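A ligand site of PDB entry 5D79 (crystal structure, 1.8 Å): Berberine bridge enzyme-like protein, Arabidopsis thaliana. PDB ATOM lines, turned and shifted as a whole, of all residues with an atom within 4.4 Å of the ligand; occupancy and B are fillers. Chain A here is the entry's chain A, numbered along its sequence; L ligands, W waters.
Water W4 bridges an oxygen (O5) of the ligand and the side-chain carboxylate (OD2) of Asp 522. Water W8 lies within hydrogen-bond range of O11 of the ligand (2.7 Å) and SG of Cys 112 (3.8 Å). Water W5 bridges O6 of the ligand (2.9 Å) and N of Thr 106 (2.9 Å). Water W6 lies within hydrogen-bond range of OG of Ser 234 (3.1 Å), O5 of the ligand (3.2 Å) and N of Gly 233 (3.3 Å). Water W2 bridges OH of Tyr 432 (2.6 Å) and OH of Tyr 113 (3.2 Å). Water W3 lies within hydrogen-bond range of O of Asn 472 (2.6 Å), N of Lys 474 (3.0 Å), N of Tyr 113 (3.0 Å) and O10 of the ligand (3.4 Å).
The backbone carbonyl oxygen (O) of Thr 149 is in hydrogen-bond range of the side-chain hydroxyl (OG) of Ser 108 (3.0 Å). The side-chain hydroxyl (OH) of Tyr 470 lies within hydrogen-bond range of the backbone NH (N) of Gly 187, 2.7 Å away. The side-chain amino group (NZ) of Lys 474 lies within hydrogen-bond range of the side-chain sulfur (SG) of Cys 112 (3.7 Å). The side-chain amino group of Lys 474 lies within salt-bridge range of the side-chain carboxylate of Asp 522 (3.4 Å). The backbone carbonyl oxygen (O) of Gly 181 lies close to the side-chain amide oxygen (OD1) of Asn 472 (3.2 Å). O of Thr 149 is in hydrogen-bond range of N of Gly 180, at 3.4 Å. The side-chain hydroxyl (OG) of Ser 184 is in hydrogen-bond range of the backbone carbonyl oxygen (O) of Gly 180 (3.0 Å). The side-chain carboxylate of Asp 522 sits at hydrogen-bond distance from the side-chain hydroxyl of Ser 234.
An oxygen (O15) of the ligand lies within hydrogen-bond range of the backbone NH (N) of His 111, at 2.9 Å. The backbone carbonyl oxygen (O) of His 111 lies within hydrogen-bond range of an oxygen (O10) of the ligand, at 3.0 Å. A ring nitrogen (ND1) of His 111 is covalently linked to a carbon (C19) of the ligand, at 1.6 Å. O1 of the ligand is in hydrogen-bond range of OG of Ser 117 (2.5 Å). N of Ser 108 is in hydrogen-bond range of O2 of the ligand (2.9 Å). OG of Ser 108 is in hydrogen-bond range of N2 of the ligand (2.6 Å). N of Gly 178 is in hydrogen-bond range of O14 of the ligand (2.7 Å). OH of Tyr 470 lies within hydrogen-bond range of O7 of the ligand, 2.7 Å away. An oxygen (O5) of the ligand lies within hydrogen-bond range of the side-chain amino group (NZ) of Lys 474, at 2.7 Å. N of Ile 239 lies within hydrogen-bond range of N4 of the ligand, 3.0 Å away. O of Ile 239 is in hydrogen-bond range of N3 of the ligand. N of Gly 110 sits at hydrogen-bond distance from O2 of the ligand (2.8 Å). O6 of the ligand is in hydrogen-bond range of O of Thr 106 (2.9 Å). An oxygen (O10) of the ligand sits close to the backbone carbonyl oxygen of Asn 472. An oxygen (O11) of the ligand is in hydrogen-bond range of the side-chain amide oxygen (OD1) of Asn 472, 3.0 Å away. N of Gly 181 lies within hydrogen-bond range of O13 of the ligand. O11 of the ligand sits close to O of Gly 181 (3.2 Å). The backbone NH of Cys 112 lies within hydrogen-bond range of an oxygen (O1) of the ligand. The backbone NH (N) of Tyr 188 lies within hydrogen-bond range of an oxygen (O7) of the ligand (3.1 Å). The backbone carbonyl oxygen (O) of Tyr 188 is in hydrogen-bond range of a nitrogen (N7) of the ligand (3.3 Å). An oxygen (O12) of the ligand lies within hydrogen-bond range of the backbone NH of Gln 182 (3.2 Å). N of Ala 109 lies within hydrogen-bond range of O2 of the ligand, 3.3 Å away. A ring nitrogen (ND1) of His 174 is in hydrogen-bond range of a nitrogen (N8) of the ligand, 3.4 Å away.
Merely in contact with the ligand: Gly 237 (3.3 Å), Leu 130 (3.4 Å), Thr 149 (3.5 Å), Gly 233 (3.5 Å), Gly 180 (3.5 Å), Phe 473 (3.5 Å), Gly 187 (3.5 Å), Ser 234 (3.5 Å), Tyr 113 (3.6 Å), Arg 107 (3.6 Å), Val 177 (3.7 Å) and Val 238 (3.9 Å). Hydrophobic or aromatic side chains that line the ligand: Ala 109, His 111, Tyr 113, Leu 130, His 174, Val 177, Tyr 188, Ile 239, Tyr 470 and Phe 473. 28 residues have an atom within 4 Å of the ligand: Thr 106, Arg 107, Ser 108, Ala 109, Gly 110, His 111, Cys 112, Tyr 113, Ser 117, Leu 130, Thr 149, His 174, Val 177, Gly 178, Gly 180, Gly 181, Gln 182, Gly 187, Tyr 188, Gly 233, Ser 234, Gly 237, Val 238, Ile 239, Tyr 470, Asn 472, Phe 473 and Lys 474. The nearest printed residue that does not touch the ligand is Asp 522 (4.1 Å).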
ATOM      1  N   THR A 106       3.629  -0.920  -8.604  1.00  0.00           N
ATOM      2  CA  THR A 106       2.964  -2.111  -9.127  1.00  0.00           C
ATOM      3  C   THR A 106       2.490  -3.051  -8.031  1.00  0.00           C
ATOM      4  O   THR A 106       3.285  -3.514  -7.204  1.00  0.00           O
ATOM      5  CB  THR A 106       3.897  -2.885 -10.064  1.00  0.00           C
ATOM      6  OG1 THR A 106       4.169  -2.090 -11.220  1.00  0.00           O
ATOM      7  CG2 THR A 106       3.231  -4.190 -10.508  1.00  0.00           C
ATOM      8  N   ARG A 107       1.202  -3.359  -8.021  1.00  0.00           N
ATOM      9  CA  ARG A 107       0.660  -4.260  -7.018  1.00  0.00           C
ATOM     10  C   ARG A 107       0.150  -5.566  -7.635  1.00  0.00           C
ATOM     11  O   ARG A 107      -0.583  -5.548  -8.619  1.00  0.00           O
ATOM     12  CB  ARG A 107      -0.476  -3.586  -6.237  1.00  0.00           C
ATOM     13  CG  ARG A 107      -1.007  -4.453  -5.116  1.00  0.00           C
ATOM     14  CD  ARG A 107      -1.810  -3.674  -4.106  1.00  0.00           C
ATOM     15  NE  ARG A 107      -3.095  -3.249  -4.634  1.00  0.00           N
ATOM     16  CZ  ARG A 107      -3.959  -2.490  -3.977  1.00  0.00           C
ATOM     17  NH1 ARG A 107      -3.662  -2.055  -2.761  1.00  0.00           N
ATOM     18  NH2 ARG A 107      -5.122  -2.175  -4.534  1.00  0.00           N
ATOM     19  N   SER A 108       0.559  -6.693  -7.052  1.00  0.00           N
ATOM     20  CA  SER A 108      -0.022  -7.986  -7.397  1.00  0.00           C
ATOM     21  C   SER A 108      -1.135  -8.355  -6.416  1.00  0.00           C
ATOM     22  O   SER A 108      -2.303  -8.219  -6.723  1.00  0.00           O
ATOM     23  CB  SER A 108       1.031  -9.088  -7.434  1.00  0.00           C
ATOM     24  OG  SER A 108       1.975  -8.845  -8.457  1.00  0.00           O
ATOM     25  N   ALA A 109      -0.772  -8.803  -5.214  1.00  0.00           N
ATOM     26  CA  ALA A 109      -1.785  -9.162  -4.237  1.00  0.00           C
ATOM     27  C   ALA A 109      -1.568  -8.427  -2.933  1.00  0.00           C
ATOM     28  O   ALA A 109      -2.293  -8.640  -1.971  1.00  0.00           O
ATOM     29  CB  ALA A 109      -1.816 -10.666  -4.010  1.00  0.00           C
ATOM     30  N   GLY A 110      -0.539  -7.582  -2.900  1.00  0.00           N
ATOM     31  CA  GLY A 110      -0.428  -6.553  -1.865  1.00  0.00           C
ATOM     32  C   GLY A 110       0.030  -6.965  -0.477  1.00  0.00           C
ATOM     33  O   GLY A 110      -0.352  -6.347   0.510  1.00  0.00           O
ATOM     34  N   HIS A 111       0.868  -7.987  -0.403  1.00  0.00           N
ATOM     35  CA  HIS A 111       1.411  -8.416   0.882  1.00  0.00           C
ATOM     36  C   HIS A 111       2.706  -7.700   1.307  1.00  0.00           C
ATOM     37  O   HIS A 111       3.326  -8.115   2.271  1.00  0.00           O
ATOM     38  CB  HIS A 111       1.643  -9.925   0.857  1.00  0.00           C
ATOM     39  CG  HIS A 111       0.455 -10.697   1.339  1.00  0.00           C
ATOM     40  ND1 HIS A 111       0.279 -11.035   2.660  1.00  0.00           N
ATOM     41  CD2 HIS A 111      -0.639 -11.175   0.681  1.00  0.00           C
ATOM     42  CE1 HIS A 111      -0.859 -11.686   2.804  1.00  0.00           C
ATOM     43  NE2 HIS A 111      -1.435 -11.785   1.619  1.00  0.00           N
ATOM     44  N   CYS A 112       3.090  -6.631   0.603  1.00  0.00           N
ATOM     45  CA  CYS A 112       4.325  -5.911   0.928  1.00  0.00           C
ATOM     46  C   CYS A 112       4.326  -5.450   2.371  1.00  0.00           C
ATOM     47  O   CYS A 112       3.434  -4.720   2.806  1.00  0.00           O
ATOM     48  CB  CYS A 112       4.530  -4.690   0.002  1.00  0.00           C
ATOM     49  SG  CYS A 112       6.208  -3.951   0.071  1.00  0.00           S
ATOM     50  N   TYR A 113       5.352  -5.875   3.098  1.00  0.00           N
ATOM     51  CA  TYR A 113       5.463  -5.653   4.536  1.00  0.00           C
ATOM     52  C   TYR A 113       5.392  -4.171   4.935  1.00  0.00           C
ATOM     53  O   TYR A 113       4.980  -3.848   6.055  1.00  0.00           O
ATOM     54  CB  TYR A 113       6.761  -6.292   5.034  1.00  0.00           C
ATOM     55  CG  TYR A 113       6.551  -7.698   5.561  1.00  0.00           C
ATOM     56  CD1 TYR A 113       5.662  -8.564   4.931  1.00  0.00           C
ATOM     57  CD2 TYR A 113       7.238  -8.144   6.681  1.00  0.00           C
ATOM     58  CE1 TYR A 113       5.445  -9.851   5.422  1.00  0.00           C
ATOM     59  CE2 TYR A 113       7.043  -9.435   7.176  1.00  0.00           C
ATOM     60  CZ  TYR A 113       6.139 -10.276   6.546  1.00  0.00           C
ATOM     61  OH  TYR A 113       5.952 -11.546   7.045  1.00  0.00           O
ATOM     62  N   SER A 117       3.794  -1.259  -2.494  1.00  0.00           N
ATOM     63  CA  SER A 117       3.156  -1.545  -3.777  1.00  0.00           C
ATOM     64  C   SER A 117       1.939  -0.638  -4.039  1.00  0.00           C
ATOM     65  O   SER A 117       1.467  -0.508  -5.172  1.00  0.00           O
ATOM     66  CB  SER A 117       2.722  -3.015  -3.829  1.00  0.00           C
ATOM     67  OG  SER A 117       1.962  -3.360  -2.695  1.00  0.00           O
ATOM     68  N   LEU A 130      -2.509  -5.540 -10.649  1.00  0.00           N
ATOM     69  CA  LEU A 130      -2.472  -6.652 -11.609  1.00  0.00           C
ATOM     70  C   LEU A 130      -3.564  -7.685 -11.392  1.00  0.00           C
ATOM     71  O   LEU A 130      -3.508  -8.768 -11.964  1.00  0.00           O
ATOM     72  CB  LEU A 130      -1.118  -7.342 -11.552  1.00  0.00           C
ATOM     73  CG  LEU A 130       0.060  -6.450 -11.929  1.00  0.00           C
ATOM     74  CD1 LEU A 130       1.364  -7.140 -11.628  1.00  0.00           C
ATOM     75  CD2 LEU A 130      -0.030  -6.077 -13.392  1.00  0.00           C
ATOM     76  N   THR A 149       1.295 -12.663 -13.301  1.00  0.00           N
ATOM     77  CA  THR A 149       1.745 -12.150 -12.004  1.00  0.00           C
ATOM     78  C   THR A 149       0.652 -11.628 -11.062  1.00  0.00           C
ATOM     79  O   THR A 149       0.927 -11.314  -9.908  1.00  0.00           O
ATOM     80  CB  THR A 149       2.765 -11.029 -12.227  1.00  0.00           C
ATOM     81  OG1 THR A 149       2.274 -10.142 -13.236  1.00  0.00           O
ATOM     82  CG2 THR A 149       4.107 -11.622 -12.666  1.00  0.00           C
ATOM     83  N   HIS A 174       1.420 -19.077   2.608  1.00  0.00           N
ATOM     84  CA  HIS A 174       0.234 -18.224   2.748  1.00  0.00           C
ATOM     85  C   HIS A 174      -0.471 -17.976   1.387  1.00  0.00           C
ATOM     86  O   HIS A 174       0.092 -17.348   0.483  1.00  0.00           O
ATOM     87  CB  HIS A 174       0.623 -16.906   3.426  1.00  0.00           C
ATOM     88  CG  HIS A 174       1.131 -17.065   4.835  1.00  0.00           C
ATOM     89  ND1 HIS A 174       2.453 -17.357   5.125  1.00  0.00           N
ATOM     90  CD2 HIS A 174       0.493 -16.982   6.024  1.00  0.00           C
ATOM     91  CE1 HIS A 174       2.609 -17.440   6.433  1.00  0.00           C
ATOM     92  NE2 HIS A 174       1.432 -17.215   7.008  1.00  0.00           N
ATOM     93  N   VAL A 177      -0.818 -14.553  -0.862  1.00  0.00           N
ATOM     94  CA  VAL A 177       0.361 -13.852  -1.304  1.00  0.00           C
ATOM     95  C   VAL A 177       0.512 -13.994  -2.819  1.00  0.00           C
ATOM     96  O   VAL A 177       0.388 -15.085  -3.369  1.00  0.00           O
ATOM     97  CB  VAL A 177       1.626 -14.374  -0.584  1.00  0.00           C
ATOM     98  CG1 VAL A 177       2.871 -13.736  -1.185  1.00  0.00           C
ATOM     99  CG2 VAL A 177       1.532 -14.083   0.899  1.00  0.00           C
ATOM    100  N   GLY A 178       0.773 -12.865  -3.484  1.00  0.00           N
ATOM    101  CA  GLY A 178       0.853 -12.842  -4.926  1.00  0.00           C
ATOM    102  C   GLY A 178       2.153 -13.404  -5.433  1.00  0.00           C
ATOM    103  O   GLY A 178       3.181 -13.303  -4.762  1.00  0.00           O
ATOM    104  N   GLY A 180       3.603 -12.236  -8.037  1.00  0.00           N
ATOM    105  CA  GLY A 180       4.349 -11.094  -8.527  1.00  0.00           C
ATOM    106  C   GLY A 180       5.425 -10.637  -7.565  1.00  0.00           C
ATOM    107  O   GLY A 180       6.602 -10.610  -7.905  1.00  0.00           O
ATOM    108  N   GLY A 181       5.020 -10.258  -6.363  1.00  0.00           N
ATOM    109  CA  GLY A 181       5.963  -9.805  -5.365  1.00  0.00           C
ATOM    110  C   GLY A 181       6.787 -10.939  -4.795  1.00  0.00           C
ATOM    111  O   GLY A 181       8.006 -10.809  -4.631  1.00  0.00           O
ATOM    112  N   GLN A 182       6.138 -12.060  -4.484  1.00  0.00           N
ATOM    113  CA  GLN A 182       6.828 -13.140  -3.793  1.00  0.00           C
ATOM    114  C   GLN A 182       7.946 -13.761  -4.657  1.00  0.00           C
ATOM    115  O   GLN A 182       9.059 -13.959  -4.175  1.00  0.00           O
ATOM    116  CB  GLN A 182       5.849 -14.232  -3.342  1.00  0.00           C
ATOM    117  CG  GLN A 182       6.538 -15.360  -2.563  1.00  0.00           C
ATOM    118  CD  GLN A 182       5.619 -16.465  -2.076  1.00  0.00           C
ATOM    119  OE1 GLN A 182       5.610 -17.562  -2.633  1.00  0.00           O
ATOM    120  NE2 GLN A 182       4.865 -16.215  -1.015  1.00  0.00           N
ATOM    121  N   SER A 184       9.458 -12.492  -7.306  1.00  0.00           N
ATOM    122  CA  SER A 184      10.505 -11.521  -7.655  1.00  0.00           C
ATOM    123  C   SER A 184      11.428 -11.207  -6.466  1.00  0.00           C
ATOM    124  O   SER A 184      12.478 -10.602  -6.646  1.00  0.00           O
ATOM    125  CB  SER A 184       9.893 -10.227  -8.217  1.00  0.00           C
ATOM    126  OG  SER A 184       9.280  -9.409  -7.228  1.00  0.00           O
ATOM    127  N   GLY A 187      11.169 -16.247  -2.247  1.00  0.00           N
ATOM    128  CA  GLY A 187       9.995 -17.056  -1.945  1.00  0.00           C
ATOM    129  C   GLY A 187      10.260 -18.433  -1.374  1.00  0.00           C
ATOM    130  O   GLY A 187      10.460 -19.384  -2.113  1.00  0.00           O
ATOM    131  N   TYR A 188      10.245 -18.559  -0.050  1.00  0.00           N
ATOM    132  CA  TYR A 188      10.442 -19.861   0.582  1.00  0.00           C
ATOM    133  C   TYR A 188       9.147 -20.371   1.215  1.00  0.00           C
ATOM    134  O   TYR A 188       8.232 -19.609   1.531  1.00  0.00           O
ATOM    135  CB  TYR A 188      11.571 -19.805   1.628  1.00  0.00           C
ATOM    136  CG  TYR A 188      11.266 -19.012   2.896  1.00  0.00           C
ATOM    137  CD1 TYR A 188      10.453 -19.523   3.903  1.00  0.00           C
ATOM    138  CD2 TYR A 188      11.830 -17.757   3.104  1.00  0.00           C
ATOM    139  CE1 TYR A 188      10.178 -18.812   5.059  1.00  0.00           C
ATOM    140  CE2 TYR A 188      11.562 -17.025   4.264  1.00  0.00           C
ATOM    141  CZ  TYR A 188      10.742 -17.566   5.237  1.00  0.00           C
ATOM    142  OH  TYR A 188      10.480 -16.840   6.385  1.00  0.00           O
ATOM    143  N   GLY A 233      11.334  -7.168  -7.776  1.00  0.00           N
ATOM    144  CA  GLY A 233      10.848  -6.713  -9.077  1.00  0.00           C
ATOM    145  C   GLY A 233      10.608  -5.221  -9.217  1.00  0.00           C
ATOM    146  O   GLY A 233      10.696  -4.691 -10.323  1.00  0.00           O
ATOM    147  N   SER A 234      10.299  -4.532  -8.120  1.00  0.00           N
ATOM    148  CA  SER A 234       9.976  -3.104  -8.217  1.00  0.00           C
ATOM    149  C   SER A 234      11.149  -2.251  -8.724  1.00  0.00           C
ATOM    150  O   SER A 234      10.961  -1.088  -9.100  1.00  0.00           O
ATOM    151  CB  SER A 234       9.507  -2.587  -6.851  1.00  0.00           C
ATOM    152  OG  SER A 234      10.524  -2.691  -5.881  1.00  0.00           O
ATOM    153  N   GLY A 237      11.207  -3.471 -13.523  1.00  0.00           N
ATOM    154  CA  GLY A 237      10.166  -3.399 -14.543  1.00  0.00           C
ATOM    155  C   GLY A 237       8.800  -3.832 -14.055  1.00  0.00           C
ATOM    156  O   GLY A 237       8.556  -3.892 -12.851  1.00  0.00           O
ATOM    157  N   VAL A 238       7.905  -4.106 -14.992  1.00  0.00           N
ATOM    158  CA  VAL A 238       6.639  -4.755 -14.651  1.00  0.00           C
ATOM    159  C   VAL A 238       6.624  -6.168 -15.198  1.00  0.00           C
ATOM    160  O   VAL A 238       6.453  -6.380 -16.401  1.00  0.00           O
ATOM    161  CB  VAL A 238       5.413  -4.008 -15.199  1.00  0.00           C
ATOM    162  CG1 VAL A 238       4.125  -4.674 -14.684  1.00  0.00           C
ATOM    163  CG2 VAL A 238       5.447  -2.545 -14.789  1.00  0.00           C
ATOM    164  N   ILE A 239       6.782  -7.132 -14.294  1.00  0.00           N
ATOM    165  CA  ILE A 239       6.785  -8.530 -14.678  1.00  0.00           C
ATOM    166  C   ILE A 239       5.353  -8.979 -14.954  1.00  0.00           C
ATOM    167  O   ILE A 239       4.465  -8.839 -14.103  1.00  0.00           O
ATOM    168  CB  ILE A 239       7.429  -9.423 -13.580  1.00  0.00           C
ATOM    169  CG1 ILE A 239       8.749  -8.798 -13.122  1.00  0.00           C
ATOM    170  CG2 ILE A 239       7.672 -10.822 -14.112  1.00  0.00           C
ATOM    171  CD1 ILE A 239       9.241  -9.314 -11.809  1.00  0.00           C
ATOM    172  N   PHE A 365       0.514  -5.904  11.007  1.00  0.00           N
ATOM    173  CA  PHE A 365       1.722  -6.513  11.540  1.00  0.00           C
ATOM    174  C   PHE A 365       2.960  -5.640  11.320  1.00  0.00           C
ATOM    175  O   PHE A 365       2.960  -4.729  10.493  1.00  0.00           O
ATOM    176  CB  PHE A 365       1.922  -7.907  10.925  1.00  0.00           C
ATOM    177  CG  PHE A 365       2.104  -7.891   9.427  1.00  0.00           C
ATOM    178  CD1 PHE A 365       3.351  -7.645   8.872  1.00  0.00           C
ATOM    179  CD2 PHE A 365       1.024  -8.117   8.587  1.00  0.00           C
ATOM    180  CE1 PHE A 365       3.518  -7.610   7.494  1.00  0.00           C
ATOM    181  CE2 PHE A 365       1.185  -8.094   7.204  1.00  0.00           C
ATOM    182  CZ  PHE A 365       2.429  -7.834   6.657  1.00  0.00           C
ATOM    183  N   TYR A 432       1.449  -9.357  15.323  1.00  0.00           N
ATOM    184  CA  TYR A 432       0.158  -9.087  14.703  1.00  0.00           C
ATOM    185  C   TYR A 432      -0.744  -8.359  15.683  1.00  0.00           C
ATOM    186  O   TYR A 432      -0.601  -8.509  16.903  1.00  0.00           O
ATOM    187  CB  TYR A 432      -0.503 -10.390  14.236  1.00  0.00           C
ATOM    188  CG  TYR A 432       0.242 -11.066  13.103  1.00  0.00           C
ATOM    189  CD1 TYR A 432       1.280 -11.948  13.357  1.00  0.00           C
ATOM    190  CD2 TYR A 432      -0.092 -10.809  11.784  1.00  0.00           C
ATOM    191  CE1 TYR A 432       1.965 -12.552  12.315  1.00  0.00           C
ATOM    192  CE2 TYR A 432       0.574 -11.407  10.747  1.00  0.00           C
ATOM    193  CZ  TYR A 432       1.609 -12.275  11.010  1.00  0.00           C
ATOM    194  OH  TYR A 432       2.286 -12.867   9.968  1.00  0.00           O
ATOM    195  N   TYR A 470      15.892 -10.689   4.571  1.00  0.00           N
ATOM    196  CA  TYR A 470      15.100 -11.220   3.463  1.00  0.00           C
ATOM    197  C   TYR A 470      14.215 -10.124   2.792  1.00  0.00           C
ATOM    198  O   TYR A 470      13.339  -9.537   3.438  1.00  0.00           O
ATOM    199  CB  TYR A 470      14.232 -12.385   3.968  1.00  0.00           C
ATOM    200  CG  TYR A 470      13.392 -13.107   2.931  1.00  0.00           C
ATOM    201  CD1 TYR A 470      13.816 -13.238   1.611  1.00  0.00           C
ATOM    202  CD2 TYR A 470      12.165 -13.666   3.280  1.00  0.00           C
ATOM    203  CE1 TYR A 470      13.030 -13.910   0.674  1.00  0.00           C
ATOM    204  CE2 TYR A 470      11.380 -14.312   2.359  1.00  0.00           C
ATOM    205  CZ  TYR A 470      11.823 -14.439   1.064  1.00  0.00           C
ATOM    206  OH  TYR A 470      11.016 -15.089   0.183  1.00  0.00           O
ATOM    207  N   ASN A 472      11.804 -10.101   0.787  1.00  0.00           N
ATOM    208  CA  ASN A 472      10.365 -10.316   0.817  1.00  0.00           C
ATOM    209  C   ASN A 472       9.760  -9.905   2.157  1.00  0.00           C
ATOM    210  O   ASN A 472       8.541  -9.757   2.276  1.00  0.00           O
ATOM    211  CB  ASN A 472      10.012 -11.769   0.494  1.00  0.00           C
ATOM    212  CG  ASN A 472       9.726 -11.990  -0.992  1.00  0.00           C
ATOM    213  OD1 ASN A 472       9.427 -11.049  -1.722  1.00  0.00           O
ATOM    214  ND2 ASN A 472       9.797 -13.226  -1.425  1.00  0.00           N
ATOM    215  N   PHE A 473      10.605  -9.716   3.163  1.00  0.00           N
ATOM    216  CA  PHE A 473      10.161  -9.072   4.404  1.00  0.00           C
ATOM    217  C   PHE A 473      10.697  -7.639   4.440  1.00  0.00           C
ATOM    218  O   PHE A 473      11.600  -7.330   5.215  1.00  0.00           O
ATOM    219  CB  PHE A 473      10.631  -9.858   5.657  1.00  0.00           C
ATOM    220  CG  PHE A 473      10.095 -11.270   5.757  1.00  0.00           C
ATOM    221  CD1 PHE A 473       8.822 -11.595   5.300  1.00  0.00           C
ATOM    222  CD2 PHE A 473      10.862 -12.282   6.341  1.00  0.00           C
ATOM    223  CE1 PHE A 473       8.326 -12.901   5.393  1.00  0.00           C
ATOM    224  CE2 PHE A 473      10.376 -13.591   6.432  1.00  0.00           C
ATOM    225  CZ  PHE A 473       9.116 -13.900   5.966  1.00  0.00           C
ATOM    226  N   LYS A 474      10.171  -6.762   3.587  1.00  0.00           N
ATOM    227  CA  LYS A 474      10.675  -5.385   3.485  1.00  0.00           C
ATOM    228  C   LYS A 474      10.634  -4.638   4.822  1.00  0.00           C
ATOM    229  O   LYS A 474       9.633  -4.675   5.537  1.00  0.00           O
ATOM    230  CB  LYS A 474       9.893  -4.591   2.425  1.00  0.00           C
ATOM    231  CG  LYS A 474      10.609  -4.417   1.085  1.00  0.00           C
ATOM    232  CD  LYS A 474       9.915  -3.359   0.249  1.00  0.00           C
ATOM    233  CE  LYS A 474       9.989  -3.670  -1.244  1.00  0.00           C
ATOM    234  NZ  LYS A 474       9.048  -2.800  -2.027  1.00  0.00           N
ATOM    235  N   ASP A 522      11.477   2.756  -5.722  1.00  0.00           N
ATOM    236  CA  ASP A 522      10.734   3.016  -4.483  1.00  0.00           C
ATOM    237  C   ASP A 522      11.721   3.464  -3.402  1.00  0.00           C
ATOM    238  O   ASP A 522      12.842   3.879  -3.703  1.00  0.00           O
ATOM    239  CB  ASP A 522       9.918   1.790  -4.037  1.00  0.00           C
ATOM    240  CG  ASP A 522      10.701   0.486  -4.052  1.00  0.00           C
ATOM    241  OD1 ASP A 522      11.904   0.478  -3.721  1.00  0.00           O
ATOM    242  OD2 ASP A 522      10.105  -0.552  -4.375  1.00  0.00           O
HETATM  243  P1  LIG L   1       2.788  -6.819  -3.377  1.00  0.00           P
HETATM  244  O1  LIG L   1       2.618  -5.768  -2.325  1.00  0.00           O
HETATM  245  O2  LIG L   1       1.706  -6.773  -4.442  1.00  0.00           O
HETATM  246  O3  LIG L   1       4.263  -6.704  -4.025  1.00  0.00           O
HETATM  247  C1  LIG L   1       5.420  -6.563  -3.203  1.00  0.00           C
HETATM  248  C2  LIG L   1       6.592  -5.923  -3.953  1.00  0.00           C
HETATM  249  O4  LIG L   1       6.765  -6.564  -5.199  1.00  0.00           O
HETATM  250  C3  LIG L   1       6.345  -4.446  -4.218  1.00  0.00           C
HETATM  251  O5  LIG L   1       7.541  -3.705  -4.133  1.00  0.00           O
HETATM  252  C4  LIG L   1       5.804  -4.454  -5.643  1.00  0.00           C
HETATM  253  O6  LIG L   1       6.074  -3.239  -6.331  1.00  0.00           O
HETATM  254  C5  LIG L   1       6.489  -5.666  -6.263  1.00  0.00           C
HETATM  255  N1  LIG L   1       5.712  -6.335  -7.323  1.00  0.00           N
HETATM  256  C6  LIG L   1       4.521  -7.018  -7.217  1.00  0.00           C
HETATM  257  N2  LIG L   1       4.187  -7.484  -8.457  1.00  0.00           N
HETATM  258  C7  LIG L   1       5.134  -7.113  -9.337  1.00  0.00           C
HETATM  259  C8  LIG L   1       5.310  -7.302 -10.709  1.00  0.00           C
HETATM  260  N3  LIG L   1       4.549  -8.183 -11.369  1.00  0.00           N
HETATM  261  N4  LIG L   1       6.413  -6.782 -11.343  1.00  0.00           N
HETATM  262  C9  LIG L   1       7.361  -6.086 -10.630  1.00  0.00           C
HETATM  263  N5  LIG L   1       7.181  -5.898  -9.267  1.00  0.00           N
HETATM  264  C10 LIG L   1       6.097  -6.391  -8.636  1.00  0.00           C
HETATM  265  N6  LIG L   1       7.249 -14.699   2.065  1.00  0.00           N
HETATM  266  C11 LIG L   1       7.950 -15.893   2.106  1.00  0.00           C
HETATM  267  O7  LIG L   1       8.771 -16.165   1.234  1.00  0.00           O
HETATM  268  N7  LIG L   1       7.694 -16.797   3.129  1.00  0.00           N
HETATM  269  C12 LIG L   1       6.757 -16.518   4.117  1.00  0.00           C
HETATM  270  O8  LIG L   1       6.475 -17.392   4.937  1.00  0.00           O
HETATM  271  C13 LIG L   1       6.036 -15.327   4.050  1.00  0.00           C
HETATM  272  N8  LIG L   1       4.997 -15.078   4.940  1.00  0.00           N
HETATM  273  C14 LIG L   1       4.110 -14.040   4.673  1.00  0.00           C
HETATM  274  C15 LIG L   1       2.921 -13.910   5.382  1.00  0.00           C
HETATM  275  C16 LIG L   1       2.036 -12.863   5.113  1.00  0.00           C
HETATM  276  C17 LIG L   1       0.770 -12.728   5.891  1.00  0.00           C
HETATM  277  C18 LIG L   1       2.321 -11.959   4.080  1.00  0.00           C
HETATM  278  C19 LIG L   1       1.402 -10.818   3.779  1.00  0.00           C
HETATM  279  C20 LIG L   1       3.509 -12.098   3.374  1.00  0.00           C
HETATM  280  C21 LIG L   1       4.424 -13.093   3.696  1.00  0.00           C
HETATM  281  N9  LIG L   1       5.624 -13.217   3.015  1.00  0.00           N
HETATM  282  C22 LIG L   1       6.271 -14.437   3.005  1.00  0.00           C
HETATM  283  C23 LIG L   1       6.177 -12.056   2.241  1.00  0.00           C
HETATM  284  C24 LIG L   1       5.726 -12.029   0.788  1.00  0.00           C
HETATM  285  O9  LIG L   1       6.288 -13.126   0.108  1.00  0.00           O
HETATM  286  C25 LIG L   1       6.195 -10.701   0.189  1.00  0.00           C
HETATM  287  O10 LIG L   1       5.497  -9.661   0.831  1.00  0.00           O
HETATM  288  C26 LIG L   1       5.888 -10.605  -1.287  1.00  0.00           C
HETATM  289  O11 LIG L   1       6.754  -9.682  -1.887  1.00  0.00           O
HETATM  290  C27 LIG L   1       4.483 -10.072  -1.474  1.00  0.00           C
HETATM  291  O12 LIG L   1       4.078 -10.302  -2.796  1.00  0.00           O
HETATM  292  P2  LIG L   1       2.655  -9.728  -3.246  1.00  0.00           P
HETATM  293  O13 LIG L   1       2.515  -9.805  -4.751  1.00  0.00           O
HETATM  294  O14 LIG L   1       1.532 -10.465  -2.567  1.00  0.00           O
HETATM  295  O15 LIG L   1       2.765  -8.241  -2.630  1.00  0.00           O
HETATM  296  O   HOH W   1      -2.485 -12.780   5.280  1.00  0.00           O
HETATM  297  O   HOH W   2       2.898 -11.280   7.937  1.00  0.00           O
HETATM  298  O   HOH W   3       7.737  -7.297   1.903  1.00  0.00           O
HETATM  299  O   HOH W   4       7.240  -1.169  -4.569  1.00  0.00           O
HETATM  300  O   HOH W   5       6.294  -0.657  -7.543  1.00  0.00           O
HETATM  301  O   HOH W   6       9.878  -5.606  -5.256  1.00  0.00           O
HETATM  302  O   HOH W   7       5.301 -15.475   8.122  1.00  0.00           O
HETATM  303  O   HOH W   8       7.533  -7.410  -0.644  1.00  0.00           O
HETATM  304  O   HOH W   9      -1.214 -10.015   5.935  1.00  0.00           O
HETATM  305  O   HOH W  10       6.518 -18.203   7.980  1.00  0.00           O
